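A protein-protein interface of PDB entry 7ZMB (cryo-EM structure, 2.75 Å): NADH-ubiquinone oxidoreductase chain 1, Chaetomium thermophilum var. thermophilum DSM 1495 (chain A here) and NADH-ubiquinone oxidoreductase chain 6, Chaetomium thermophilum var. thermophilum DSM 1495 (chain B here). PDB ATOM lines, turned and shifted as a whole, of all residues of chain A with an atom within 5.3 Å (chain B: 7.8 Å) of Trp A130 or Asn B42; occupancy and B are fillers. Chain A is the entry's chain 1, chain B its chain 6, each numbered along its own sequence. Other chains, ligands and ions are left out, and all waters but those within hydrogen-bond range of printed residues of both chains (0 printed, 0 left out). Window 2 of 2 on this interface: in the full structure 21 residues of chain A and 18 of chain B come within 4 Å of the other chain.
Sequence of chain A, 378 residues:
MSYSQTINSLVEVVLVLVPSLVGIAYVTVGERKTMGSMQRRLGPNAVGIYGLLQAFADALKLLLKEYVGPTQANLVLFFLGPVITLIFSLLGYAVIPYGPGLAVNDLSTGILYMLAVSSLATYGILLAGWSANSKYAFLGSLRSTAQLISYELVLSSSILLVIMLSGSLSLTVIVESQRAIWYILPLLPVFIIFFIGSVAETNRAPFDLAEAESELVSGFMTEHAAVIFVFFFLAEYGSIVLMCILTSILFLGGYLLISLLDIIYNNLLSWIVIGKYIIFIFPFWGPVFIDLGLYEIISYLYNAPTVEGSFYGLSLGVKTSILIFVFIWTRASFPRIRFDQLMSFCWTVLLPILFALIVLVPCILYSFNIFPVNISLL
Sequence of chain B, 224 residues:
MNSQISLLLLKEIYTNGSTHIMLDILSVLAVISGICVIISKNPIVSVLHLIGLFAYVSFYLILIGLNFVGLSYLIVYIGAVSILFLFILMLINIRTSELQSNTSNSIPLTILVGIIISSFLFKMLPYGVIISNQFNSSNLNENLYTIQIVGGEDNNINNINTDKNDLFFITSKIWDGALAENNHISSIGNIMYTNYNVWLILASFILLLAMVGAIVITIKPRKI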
ATOM      1  N   ASN A  74     -30.668   9.367 -30.090  1.00  0.00           N
ATOM      2  CA  ASN A  74     -29.619   8.591 -30.795  1.00  0.00           C
ATOM      3  C   ASN A  74     -30.345   7.318 -31.238  1.00  0.00           C
ATOM      4  O   ASN A  74     -30.440   6.414 -30.404  1.00  0.00           O
ATOM      5  CB  ASN A  74     -28.468   8.298 -29.839  1.00  0.00           C
ATOM      6  CG  ASN A  74     -27.523   9.469 -29.748  1.00  0.00           C
ATOM      7  OD1 ASN A  74     -27.084   9.847 -28.668  1.00  0.00           O
ATOM      8  ND2 ASN A  74     -27.232  10.071 -30.887  1.00  0.00           N
ATOM      9  N   LEU A  77     -29.065   3.410 -30.978  1.00  0.00           N
ATOM     10  CA  LEU A  77     -29.137   2.991 -29.585  1.00  0.00           C
ATOM     11  C   LEU A  77     -30.578   2.957 -29.090  1.00  0.00           C
ATOM     12  O   LEU A  77     -30.923   2.132 -28.237  1.00  0.00           O
ATOM     13  CB  LEU A  77     -28.294   3.917 -28.712  1.00  0.00           C
ATOM     14  CG  LEU A  77     -26.873   4.268 -29.160  1.00  0.00           C
ATOM     15  CD1 LEU A  77     -26.117   4.884 -28.001  1.00  0.00           C
ATOM     16  CD2 LEU A  77     -26.122   3.057 -29.698  1.00  0.00           C
ATOM     17  N   ILE A 125     -31.772  -1.145 -20.536  1.00  0.00           N
ATOM     18  CA  ILE A 125     -32.641  -0.097 -19.926  1.00  0.00           C
ATOM     19  C   ILE A 125     -31.839   1.207 -19.836  1.00  0.00           C
ATOM     20  O   ILE A 125     -32.345   2.233 -20.319  1.00  0.00           O
ATOM     21  CB  ILE A 125     -33.143  -0.547 -18.546  1.00  0.00           C
ATOM     22  CG1 ILE A 125     -34.108  -1.730 -18.654  1.00  0.00           C
ATOM     23  CG2 ILE A 125     -33.754   0.616 -17.783  1.00  0.00           C
ATOM     24  CD1 ILE A 125     -34.656  -2.195 -17.328  1.00  0.00           C
ATOM     25  N   LEU A 126     -30.635   1.157 -19.256  1.00  0.00           N
ATOM     26  CA  LEU A 126     -29.820   2.358 -19.139  1.00  0.00           C
ATOM     27  C   LEU A 126     -29.598   3.015 -20.493  1.00  0.00           C
ATOM     28  O   LEU A 126     -29.716   4.234 -20.627  1.00  0.00           O
ATOM     29  CB  LEU A 126     -28.480   2.008 -18.493  1.00  0.00           C
ATOM     30  CG  LEU A 126     -27.361   3.047 -18.499  1.00  0.00           C
ATOM     31  CD1 LEU A 126     -27.812   4.355 -17.852  1.00  0.00           C
ATOM     32  CD2 LEU A 126     -26.139   2.489 -17.796  1.00  0.00           C
ATOM     33  N   LEU A 127     -29.284   2.218 -21.510  1.00  0.00           N
ATOM     34  CA  LEU A 127     -28.960   2.781 -22.812  1.00  0.00           C
ATOM     35  C   LEU A 127     -30.194   3.357 -23.485  1.00  0.00           C
ATOM     36  O   LEU A 127     -30.153   4.465 -24.031  1.00  0.00           O
ATOM     37  CB  LEU A 127     -28.306   1.714 -23.689  1.00  0.00           C
ATOM     38  CG  LEU A 127     -27.784   2.239 -25.021  1.00  0.00           C
ATOM     39  CD1 LEU A 127     -26.415   2.847 -24.839  1.00  0.00           C
ATOM     40  CD2 LEU A 127     -27.763   1.140 -26.074  1.00  0.00           C
ATOM     41  N   ALA A 128     -31.302   2.619 -23.458  1.00  0.00           N
ATOM     42  CA  ALA A 128     -32.519   3.087 -24.108  1.00  0.00           C
ATOM     43  C   ALA A 128     -33.019   4.378 -23.477  1.00  0.00           C
ATOM     44  O   ALA A 128     -33.427   5.304 -24.186  1.00  0.00           O
ATOM     45  CB  ALA A 128     -33.594   2.002 -24.056  1.00  0.00           C
ATOM     46  N   GLY A 129     -32.984   4.462 -22.148  1.00  0.00           N
ATOM     47  CA  GLY A 129     -33.413   5.681 -21.485  1.00  0.00           C
ATOM     48  C   GLY A 129     -32.555   6.878 -21.845  1.00  0.00           C
ATOM     49  O   GLY A 129     -33.068   7.947 -22.176  1.00  0.00           O
ATOM     50  N   TRP A 130     -31.232   6.711 -21.801  1.00  0.00           N
ATOM     51  CA  TRP A 130     -30.344   7.805 -22.167  1.00  0.00           C
ATOM     52  C   TRP A 130     -30.522   8.195 -23.628  1.00  0.00           C
ATOM     53  O   TRP A 130     -30.525   9.383 -23.965  1.00  0.00           O
ATOM     54  CB  TRP A 130     -28.890   7.429 -21.896  1.00  0.00           C
ATOM     55  CG  TRP A 130     -27.929   8.518 -22.295  1.00  0.00           C
ATOM     56  CD1 TRP A 130     -27.532   9.576 -21.535  1.00  0.00           C
ATOM     57  CD2 TRP A 130     -27.277   8.666 -23.557  1.00  0.00           C
ATOM     58  NE1 TRP A 130     -26.666  10.364 -22.240  1.00  0.00           N
ATOM     59  CE2 TRP A 130     -26.487   9.827 -23.484  1.00  0.00           C
ATOM     60  CE3 TRP A 130     -27.279   7.928 -24.742  1.00  0.00           C
ATOM     61  CZ2 TRP A 130     -25.714  10.270 -24.550  1.00  0.00           C
ATOM     62  CZ3 TRP A 130     -26.506   8.365 -25.793  1.00  0.00           C
ATOM     63  CH2 TRP A 130     -25.735   9.524 -25.692  1.00  0.00           C
ATOM     64  N   SER A 131     -30.688   7.203 -24.504  1.00  0.00           N
ATOM     65  CA  SER A 131     -30.723   7.444 -25.940  1.00  0.00           C
ATOM     66  C   SER A 131     -31.890   8.330 -26.348  1.00  0.00           C
ATOM     67  O   SER A 131     -31.809   9.029 -27.359  1.00  0.00           O
ATOM     68  CB  SER A 131     -30.807   6.113 -26.680  1.00  0.00           C
ATOM     69  OG  SER A 131     -29.844   5.214 -26.187  1.00  0.00           O
ATOM     70  N   ALA A 132     -32.976   8.306 -25.577  1.00  0.00           N
ATOM     71  CA  ALA A 132     -34.183   9.041 -25.933  1.00  0.00           C
ATOM     72  C   ALA A 132     -33.946  10.542 -25.967  1.00  0.00           C
ATOM     73  O   ALA A 132     -34.582  11.251 -26.753  1.00  0.00           O
ATOM     74  CB  ALA A 132     -35.295   8.709 -24.946  1.00  0.00           C
ATOM     75  N   ASN A 133     -33.043  11.041 -25.130  1.00  0.00           N
ATOM     76  CA  ASN A 133     -32.725  12.462 -25.071  1.00  0.00           C
ATOM     77  C   ASN A 133     -33.967  13.288 -24.733  1.00  0.00           C
ATOM     78  O   ASN A 133     -34.208  14.353 -25.301  1.00  0.00           O
ATOM     79  CB  ASN A 133     -32.074  12.926 -26.376  1.00  0.00           C
ATOM     80  CG  ASN A 133     -31.325  14.219 -26.223  1.00  0.00           C
ATOM     81  OD1 ASN A 133     -31.621  15.021 -25.348  1.00  0.00           O
ATOM     82  ND2 ASN A 133     -30.348  14.434 -27.084  1.00  0.00           N
ATOM     83  N   ALA A 137     -37.191  10.299 -19.553  1.00  0.00           N
ATOM     84  CA  ALA A 137     -36.441   9.092 -19.881  1.00  0.00           C
ATOM     85  C   ALA A 137     -35.010   9.175 -19.374  1.00  0.00           C
ATOM     86  O   ALA A 137     -34.429   8.157 -18.991  1.00  0.00           O
ATOM     87  CB  ALA A 137     -36.464   8.851 -21.386  1.00  0.00           C
ATOM     88  N   PHE A 138     -34.424  10.374 -19.376  1.00  0.00           N
ATOM     89  CA  PHE A 138     -33.106  10.548 -18.787  1.00  0.00           C
ATOM     90  C   PHE A 138     -33.140  10.303 -17.284  1.00  0.00           C
ATOM     91  O   PHE A 138     -32.251   9.641 -16.738  1.00  0.00           O
ATOM     92  CB  PHE A 138     -32.574  11.946 -19.102  1.00  0.00           C
ATOM     93  CG  PHE A 138     -31.234  12.244 -18.482  1.00  0.00           C
ATOM     94  CD1 PHE A 138     -30.069  11.839 -19.099  1.00  0.00           C
ATOM     95  CD2 PHE A 138     -31.146  12.932 -17.281  1.00  0.00           C
ATOM     96  CE1 PHE A 138     -28.847  12.107 -18.538  1.00  0.00           C
ATOM     97  CE2 PHE A 138     -29.929  13.202 -16.717  1.00  0.00           C
ATOM     98  CZ  PHE A 138     -28.771  12.785 -17.348  1.00  0.00           C
ATOM     99  N   SER A 141     -33.541   6.490 -16.628  1.00  0.00           N
ATOM    100  CA  SER A 141     -32.364   5.646 -16.809  1.00  0.00           C
ATOM    101  C   SER A 141     -31.394   5.788 -15.641  1.00  0.00           C
ATOM    102  O   SER A 141     -30.766   4.810 -15.228  1.00  0.00           O
ATOM    103  CB  SER A 141     -31.669   5.971 -18.135  1.00  0.00           C
ATOM    104  OG  SER A 141     -30.849   7.124 -18.042  1.00  0.00           O
ATOM    105  N   CYS B  36     -13.493   1.096 -32.411  1.00  0.00           N
ATOM    106  CA  CYS B  36     -14.600   2.028 -32.261  1.00  0.00           C
ATOM    107  C   CYS B  36     -14.654   2.663 -30.879  1.00  0.00           C
ATOM    108  O   CYS B  36     -15.265   3.721 -30.731  1.00  0.00           O
ATOM    109  CB  CYS B  36     -15.921   1.328 -32.565  1.00  0.00           C
ATOM    110  SG  CYS B  36     -16.288   1.081 -34.317  1.00  0.00           S
ATOM    111  N   VAL B  37     -14.019   2.058 -29.874  1.00  0.00           N
ATOM    112  CA  VAL B  37     -13.977   2.662 -28.545  1.00  0.00           C
ATOM    113  C   VAL B  37     -13.216   3.983 -28.560  1.00  0.00           C
ATOM    114  O   VAL B  37     -13.494   4.878 -27.755  1.00  0.00           O
ATOM    115  CB  VAL B  37     -13.374   1.666 -27.532  1.00  0.00           C
ATOM    116  CG1 VAL B  37     -13.199   2.303 -26.172  1.00  0.00           C
ATOM    117  CG2 VAL B  37     -14.271   0.447 -27.401  1.00  0.00           C
ATOM    118  N   ILE B  39     -12.190   5.742 -31.783  1.00  0.00           N
ATOM    119  CA  ILE B  39     -12.447   6.609 -32.929  1.00  0.00           C
ATOM    120  C   ILE B  39     -13.814   7.274 -32.881  1.00  0.00           C
ATOM    121  O   ILE B  39     -14.041   8.246 -33.615  1.00  0.00           O
ATOM    122  CB  ILE B  39     -12.313   5.853 -34.268  1.00  0.00           C
ATOM    123  CG1 ILE B  39     -13.465   4.863 -34.453  1.00  0.00           C
ATOM    124  CG2 ILE B  39     -10.966   5.162 -34.363  1.00  0.00           C
ATOM    125  CD1 ILE B  39     -13.461   4.183 -35.788  1.00  0.00           C
ATOM    126  N   SER B  40     -14.724   6.803 -32.036  1.00  0.00           N
ATOM    127  CA  SER B  40     -16.087   7.314 -32.020  1.00  0.00           C
ATOM    128  C   SER B  40     -16.142   8.714 -31.428  1.00  0.00           C
ATOM    129  O   SER B  40     -15.441   9.026 -30.468  1.00  0.00           O
ATOM    130  CB  SER B  40     -16.997   6.382 -31.226  1.00  0.00           C
ATOM    131  OG  SER B  40     -17.373   5.261 -32.001  1.00  0.00           O
ATOM    132  N   LYS B  41     -16.999   9.556 -32.000  1.00  0.00           N
ATOM    133  CA  LYS B  41     -17.085  10.940 -31.553  1.00  0.00           C
ATOM    134  C   LYS B  41     -17.956  11.089 -30.315  1.00  0.00           C
ATOM    135  O   LYS B  41     -17.803  12.063 -29.573  1.00  0.00           O
ATOM    136  CB  LYS B  41     -17.606  11.815 -32.694  1.00  0.00           C
ATOM    137  CG  LYS B  41     -16.600  11.951 -33.828  1.00  0.00           C
ATOM    138  CD  LYS B  41     -17.153  12.697 -35.038  1.00  0.00           C
ATOM    139  CE  LYS B  41     -17.347  14.176 -34.768  1.00  0.00           C
ATOM    140  NZ  LYS B  41     -17.776  14.897 -35.998  1.00  0.00           N
ATOM    141  N   ASN B  42     -18.844  10.145 -30.067  1.00  0.00           N
ATOM    142  CA  ASN B  42     -19.744  10.245 -28.928  1.00  0.00           C
ATOM    143  C   ASN B  42     -19.285   9.319 -27.808  1.00  0.00           C
ATOM    144  O   ASN B  42     -19.028   8.134 -28.056  1.00  0.00           O
ATOM    145  CB  ASN B  42     -21.169   9.907 -29.355  1.00  0.00           C
ATOM    146  CG  ASN B  42     -22.121   9.797 -28.192  1.00  0.00           C
ATOM    147  OD1 ASN B  42     -22.489   8.708 -27.778  1.00  0.00           O
ATOM    148  ND2 ASN B  42     -22.499  10.930 -27.636  1.00  0.00           N
ATOM    149  N   PRO B  43     -19.133   9.821 -26.578  1.00  0.00           N
ATOM    150  CA  PRO B  43     -18.594   8.987 -25.490  1.00  0.00           C
ATOM    151  C   PRO B  43     -19.495   7.848 -25.060  1.00  0.00           C
ATOM    152  O   PRO B  43     -19.027   6.962 -24.339  1.00  0.00           O
ATOM    153  CB  PRO B  43     -18.407   9.990 -24.347  1.00  0.00           C
ATOM    154  CG  PRO B  43     -18.327  11.297 -25.019  1.00  0.00           C
ATOM    155  CD  PRO B  43     -19.266  11.220 -26.160  1.00  0.00           C
ATOM    156  N   ILE B  44     -20.762   7.843 -25.453  1.00  0.00           N
ATOM    157  CA  ILE B  44     -21.640   6.756 -25.052  1.00  0.00           C
ATOM    158  C   ILE B  44     -21.616   5.603 -26.053  1.00  0.00           C
ATOM    159  O   ILE B  44     -21.707   4.438 -25.653  1.00  0.00           O
ATOM    160  CB  ILE B  44     -23.063   7.284 -24.819  1.00  0.00           C
ATOM    161  CG1 ILE B  44     -23.038   8.385 -23.760  1.00  0.00           C
ATOM    162  CG2 ILE B  44     -23.978   6.185 -24.358  1.00  0.00           C
ATOM    163  CD1 ILE B  44     -22.775   7.894 -22.369  1.00  0.00           C
ATOM    164  N   VAL B  45     -21.484   5.885 -27.350  1.00  0.00           N
ATOM    165  CA  VAL B  45     -21.231   4.785 -28.270  1.00  0.00           C
ATOM    166  C   VAL B  45     -19.834   4.236 -28.036  1.00  0.00           C
ATOM    167  O   VAL B  45     -19.589   3.042 -28.226  1.00  0.00           O
ATOM    168  CB  VAL B  45     -21.439   5.213 -29.734  1.00  0.00           C
ATOM    169  CG1 VAL B  45     -22.907   5.489 -30.000  1.00  0.00           C
ATOM    170  CG2 VAL B  45     -20.583   6.404 -30.083  1.00  0.00           C
ATOM    171  N   SER B  46     -18.905   5.091 -27.605  1.00  0.00           N
ATOM    172  CA  SER B  46     -17.563   4.632 -27.271  1.00  0.00           C
ATOM    173  C   SER B  46     -17.589   3.645 -26.112  1.00  0.00           C
ATOM    174  O   SER B  46     -16.870   2.641 -26.127  1.00  0.00           O
ATOM    175  CB  SER B  46     -16.673   5.829 -26.939  1.00  0.00           C
ATOM    176  OG  SER B  46     -15.452   5.418 -26.359  1.00  0.00           O
ATOM    177  N   VAL B  47     -18.405   3.917 -25.094  1.00  0.00           N
ATOM    178  CA  VAL B  47     -18.492   3.008 -23.958  1.00  0.00           C
ATOM    179  C   VAL B  47     -19.406   1.831 -24.258  1.00  0.00           C
ATOM    180  O   VAL B  47     -19.256   0.771 -23.642  1.00  0.00           O
ATOM    181  CB  VAL B  47     -18.928   3.766 -22.686  1.00  0.00           C
ATOM    182  CG1 VAL B  47     -20.418   4.122 -22.718  1.00  0.00           C
ATOM    183  CG2 VAL B  47     -18.587   2.973 -21.446  1.00  0.00           C
ATOM    184  N   LEU B  48     -20.351   1.980 -25.191  1.00  0.00           N
ATOM    185  CA  LEU B  48     -21.110   0.829 -25.668  1.00  0.00           C
ATOM    186  C   LEU B  48     -20.206  -0.170 -26.378  1.00  0.00           C
ATOM    187  O   LEU B  48     -20.342  -1.382 -26.193  1.00  0.00           O
ATOM    188  CB  LEU B  48     -22.224   1.277 -26.609  1.00  0.00           C
ATOM    189  CG  LEU B  48     -23.006   0.138 -27.282  1.00  0.00           C
ATOM    190  CD1 LEU B  48     -23.873  -0.640 -26.311  1.00  0.00           C
ATOM    191  CD2 LEU B  48     -23.818   0.625 -28.453  1.00  0.00           C
ATOM    192  N   HIS B  49     -19.298   0.321 -27.222  1.00  0.00           N
ATOM    193  CA  HIS B  49     -18.336  -0.563 -27.861  1.00  0.00           C
ATOM    194  C   HIS B  49     -17.408  -1.186 -26.835  1.00  0.00           C
ATOM    195  O   HIS B  49     -16.886  -2.283 -27.053  1.00  0.00           O
ATOM    196  CB  HIS B  49     -17.530   0.201 -28.906  1.00  0.00           C
ATOM    197  CG  HIS B  49     -18.257   0.421 -30.194  1.00  0.00           C
ATOM    198  ND1 HIS B  49     -18.305  -0.525 -31.191  1.00  0.00           N
ATOM    199  CD2 HIS B  49     -18.952   1.487 -30.653  1.00  0.00           C
ATOM    200  CE1 HIS B  49     -19.011  -0.056 -32.204  1.00  0.00           C
ATOM    201  NE2 HIS B  49     -19.407   1.166 -31.906  1.00  0.00           N
ATOM    202  N   PHE B  85     -20.334   4.548 -17.625  1.00  0.00           N
ATOM    203  CA  PHE B  85     -21.451   5.284 -18.203  1.00  0.00           C
ATOM    204  C   PHE B  85     -21.901   6.392 -17.263  1.00  0.00           C
ATOM    205  O   PHE B  85     -22.071   7.547 -17.667  1.00  0.00           O
ATOM    206  CB  PHE B  85     -22.592   4.300 -18.471  1.00  0.00           C
ATOM    207  CG  PHE B  85     -23.687   4.828 -19.351  1.00  0.00           C
ATOM    208  CD1 PHE B  85     -24.580   5.777 -18.890  1.00  0.00           C
ATOM    209  CD2 PHE B  85     -23.872   4.313 -20.612  1.00  0.00           C
ATOM    210  CE1 PHE B  85     -25.590   6.240 -19.691  1.00  0.00           C
ATOM    211  CE2 PHE B  85     -24.886   4.767 -21.407  1.00  0.00           C
ATOM    212  CZ  PHE B  85     -25.746   5.739 -20.945  1.00  0.00           C
ATOM    213  N   ILE B  88     -19.515   9.384 -17.274  1.00  0.00           N
ATOM    214  CA  ILE B  88     -19.556  10.181 -18.497  1.00  0.00           C
ATOM    215  C   ILE B  88     -20.715  11.167 -18.454  1.00  0.00           C
ATOM    216  O   ILE B  88     -20.589  12.315 -18.890  1.00  0.00           O
ATOM    217  CB  ILE B  88     -19.637   9.267 -19.730  1.00  0.00           C
ATOM    218  CG1 ILE B  88     -18.326   8.506 -19.915  1.00  0.00           C
ATOM    219  CG2 ILE B  88     -19.956  10.076 -20.967  1.00  0.00           C
ATOM    220  CD1 ILE B  88     -18.507   7.136 -20.462  1.00  0.00           C
ATOM    221  N   LEU B  89     -21.860  10.739 -17.926  1.00  0.00           N
ATOM    222  CA  LEU B  89     -23.014  11.626 -17.839  1.00  0.00           C
ATOM    223  C   LEU B  89     -22.727  12.815 -16.936  1.00  0.00           C
ATOM    224  O   LEU B  89     -23.130  13.943 -17.234  1.00  0.00           O
ATOM    225  CB  LEU B  89     -24.231  10.857 -17.331  1.00  0.00           C
ATOM    226  CG  LEU B  89     -24.782   9.774 -18.248  1.00  0.00           C
ATOM    227  CD1 LEU B  89     -26.218   9.455 -17.901  1.00  0.00           C
ATOM    228  CD2 LEU B  89     -24.654  10.200 -19.682  1.00  0.00           C
ATOM    229  N   ILE B  92     -18.830  14.809 -18.485  1.00  0.00           N
ATOM    230  CA  ILE B  92     -18.546  15.110 -19.881  1.00  0.00           C
ATOM    231  C   ILE B  92     -19.752  15.822 -20.462  1.00  0.00           C
ATOM    232  O   ILE B  92     -20.890  15.405 -20.230  1.00  0.00           O
ATOM    233  CB  ILE B  92     -18.225  13.835 -20.688  1.00  0.00           C
ATOM    234  CG1 ILE B  92     -16.844  13.301 -20.324  1.00  0.00           C
ATOM    235  CG2 ILE B  92     -18.297  14.096 -22.177  1.00  0.00           C
ATOM    236  CD1 ILE B  92     -16.609  11.892 -20.786  1.00  0.00           C
ATOM    237  N   ASN B  93     -19.508  16.907 -21.185  1.00  0.00           N
ATOM    238  CA  ASN B  93     -20.539  17.488 -22.035  1.00  0.00           C
ATOM    239  C   ASN B  93     -20.619  16.646 -23.303  1.00  0.00           C
ATOM    240  O   ASN B  93     -19.700  16.668 -24.126  1.00  0.00           O
ATOM    241  CB  ASN B  93     -20.233  18.947 -22.356  1.00  0.00           C
ATOM    242  CG  ASN B  93     -21.475  19.737 -22.720  1.00  0.00           C
ATOM    243  OD1 ASN B  93     -22.226  19.359 -23.613  1.00  0.00           O
ATOM    244  ND2 ASN B  93     -21.684  20.848 -22.040  1.00  0.00           N
ATOM    245  N   ILE B  94     -21.712  15.893 -23.450  1.00  0.00           N
ATOM    246  CA  ILE B  94     -21.856  14.993 -24.592  1.00  0.00           C
ATOM    247  C   ILE B  94     -21.856  15.769 -25.900  1.00  0.00           C
ATOM    248  O   ILE B  94     -21.206  15.370 -26.871  1.00  0.00           O
ATOM    249  CB  ILE B  94     -23.130  14.135 -24.451  1.00  0.00           C
ATOM    250  CG1 ILE B  94     -22.964  13.077 -23.363  1.00  0.00           C
ATOM    251  CG2 ILE B  94     -23.487  13.487 -25.779  1.00  0.00           C
ATOM    252  CD1 ILE B  94     -21.922  12.044 -23.689  1.00  0.00           C
ATOM    253  N   ARG B  95     -22.614  16.868 -25.958  1.00  0.00           N
ATOM    254  CA  ARG B  95     -22.756  17.578 -27.261  1.00  0.00           C
ATOM    255  C   ARG B  95     -21.416  18.178 -27.690  1.00  0.00           C
ATOM    256  O   ARG B  95     -21.029  17.944 -28.847  1.00  0.00           O
ATOM    257  CB  ARG B  95     -23.903  18.591 -27.256  1.00  0.00           C
ATOM    258  CG  ARG B  95     -24.414  18.940 -28.646  1.00  0.00           C
ATOM    259  CD  ARG B  95     -25.412  20.078 -28.619  1.00  0.00           C
ATOM    260  NE  ARG B  95     -24.820  21.282 -28.054  1.00  0.00           N
ATOM    261  CZ  ARG B  95     -25.455  22.439 -27.923  1.00  0.00           C
ATOM    262  NH1 ARG B  95     -26.711  22.554 -28.319  1.00  0.00           N
ATOM    263  NH2 ARG B  95     -24.831  23.478 -27.397  1.00  0.00           N
ATOM    264  N   SER B  97     -18.484  17.320 -26.947  1.00  0.00           N
ATOM    265  CA  SER B  97     -17.511  16.283 -27.272  1.00  0.00           C
ATOM    266  C   SER B  97     -17.806  15.637 -28.623  1.00  0.00           C
ATOM    267  O   SER B  97     -16.883  15.247 -29.343  1.00  0.00           O
ATOM    268  CB  SER B  97     -17.464  15.238 -26.158  1.00  0.00           C
ATOM    269  OG  SER B  97     -18.469  14.268 -26.320  1.00  0.00           O
ATOM    270  N   GLU B  98     -19.080  15.513 -28.993  1.00  0.00           N
ATOM    271  CA  GLU B  98     -19.387  15.040 -30.342  1.00  0.00           C
ATOM    272  C   GLU B  98     -18.957  16.032 -31.409  1.00  0.00           C
ATOM    273  O   GLU B  98     -18.977  15.690 -32.594  1.00  0.00           O
ATOM    274  CB  GLU B  98     -20.877  14.757 -30.501  1.00  0.00           C
ATOM    275  CG  GLU B  98     -21.357  13.536 -29.780  1.00  0.00           C
ATOM    276  CD  GLU B  98     -22.858  13.379 -29.863  1.00  0.00           C
ATOM    277  OE1 GLU B  98     -23.574  14.389 -29.686  1.00  0.00           O
ATOM    278  OE2 GLU B  98     -23.324  12.248 -30.119  1.00  0.00           O
ATOM    279  N   LEU B  99     -18.611  17.250 -31.012  1.00  0.00           N
ATOM    280  CA  LEU B  99     -18.022  18.251 -31.883  1.00  0.00           C
ATOM    281  C   LEU B  99     -16.511  18.315 -31.731  1.00  0.00           C
ATOM    282  O   LEU B  99     -15.860  19.137 -32.381  1.00  0.00           O
ATOM    283  CB  LEU B  99     -18.647  19.610 -31.575  1.00  0.00           C
ATOM    284  CG  LEU B  99     -20.153  19.550 -31.780  1.00  0.00           C
ATOM    285  CD1 LEU B  99     -20.891  20.628 -31.016  1.00  0.00           C
ATOM    286  CD2 LEU B  99     -20.360  19.699 -33.248  1.00  0.00           C
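The backbone NH (N) of Ile B44 sits at hydrogen-bond distance from the side-chain amide oxygen (OD1) of Asn B42 (3.0 Å).
The side-chain carboxylate of Glu B98 lies within hydrogen-bond range of the side-chain amide nitrogen of Asn B42 (2.9 Å).
The backbone NH (N) of Val B45 sits at hydrogen-bond distance from the side-chain amide oxygen (OD1) of Asn B42.
The side-chain hydroxyl of Ser A141 sits at hydrogen-bond distance from the backbone carbonyl oxygen of Phe A138 (3.2 Å).
Among the printed residues, pairs that only touch across the chains: Trp A130 with Leu B89, Trp A130 with Ile B44, Leu A126 with Phe B85, Leu A77 with Leu B48, Trp A130 with Phe B85, Phe A138 with Leu B89, Leu A77 with Val B45 and Trp A130 with Asn B42.
Of chain B, only Asn B42 (3.9 Å), Ile B44 (3.4 Å), Phe B85 (3.7 Å) and Leu B89 (3.3 Å) come within 4 Å of Trp A130.
Of the printed residues of chain A, Asn B42 touches Trp A130 (3.9 Å).
No residue of chain B comes within 4 Å of Gly A129.
Printed residues of chain B within 4 Å of Leu A77: Val B45 and Leu B48.
Of the printed residues of chain B, Leu A126 touches Phe B85.
Of the printed residues of chain A, Phe B85 touches Leu A126 and Trp A130.
Printed residues of chain A within 4 Å of Leu B48: Leu A77.
Ile B88 touches none of the printed residues of chain A.
Ser B46 touches none of the printed residues of chain A.
The nearest residue of chain B that does not touch Trp A130 is Ile B94 (4.1 Å).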
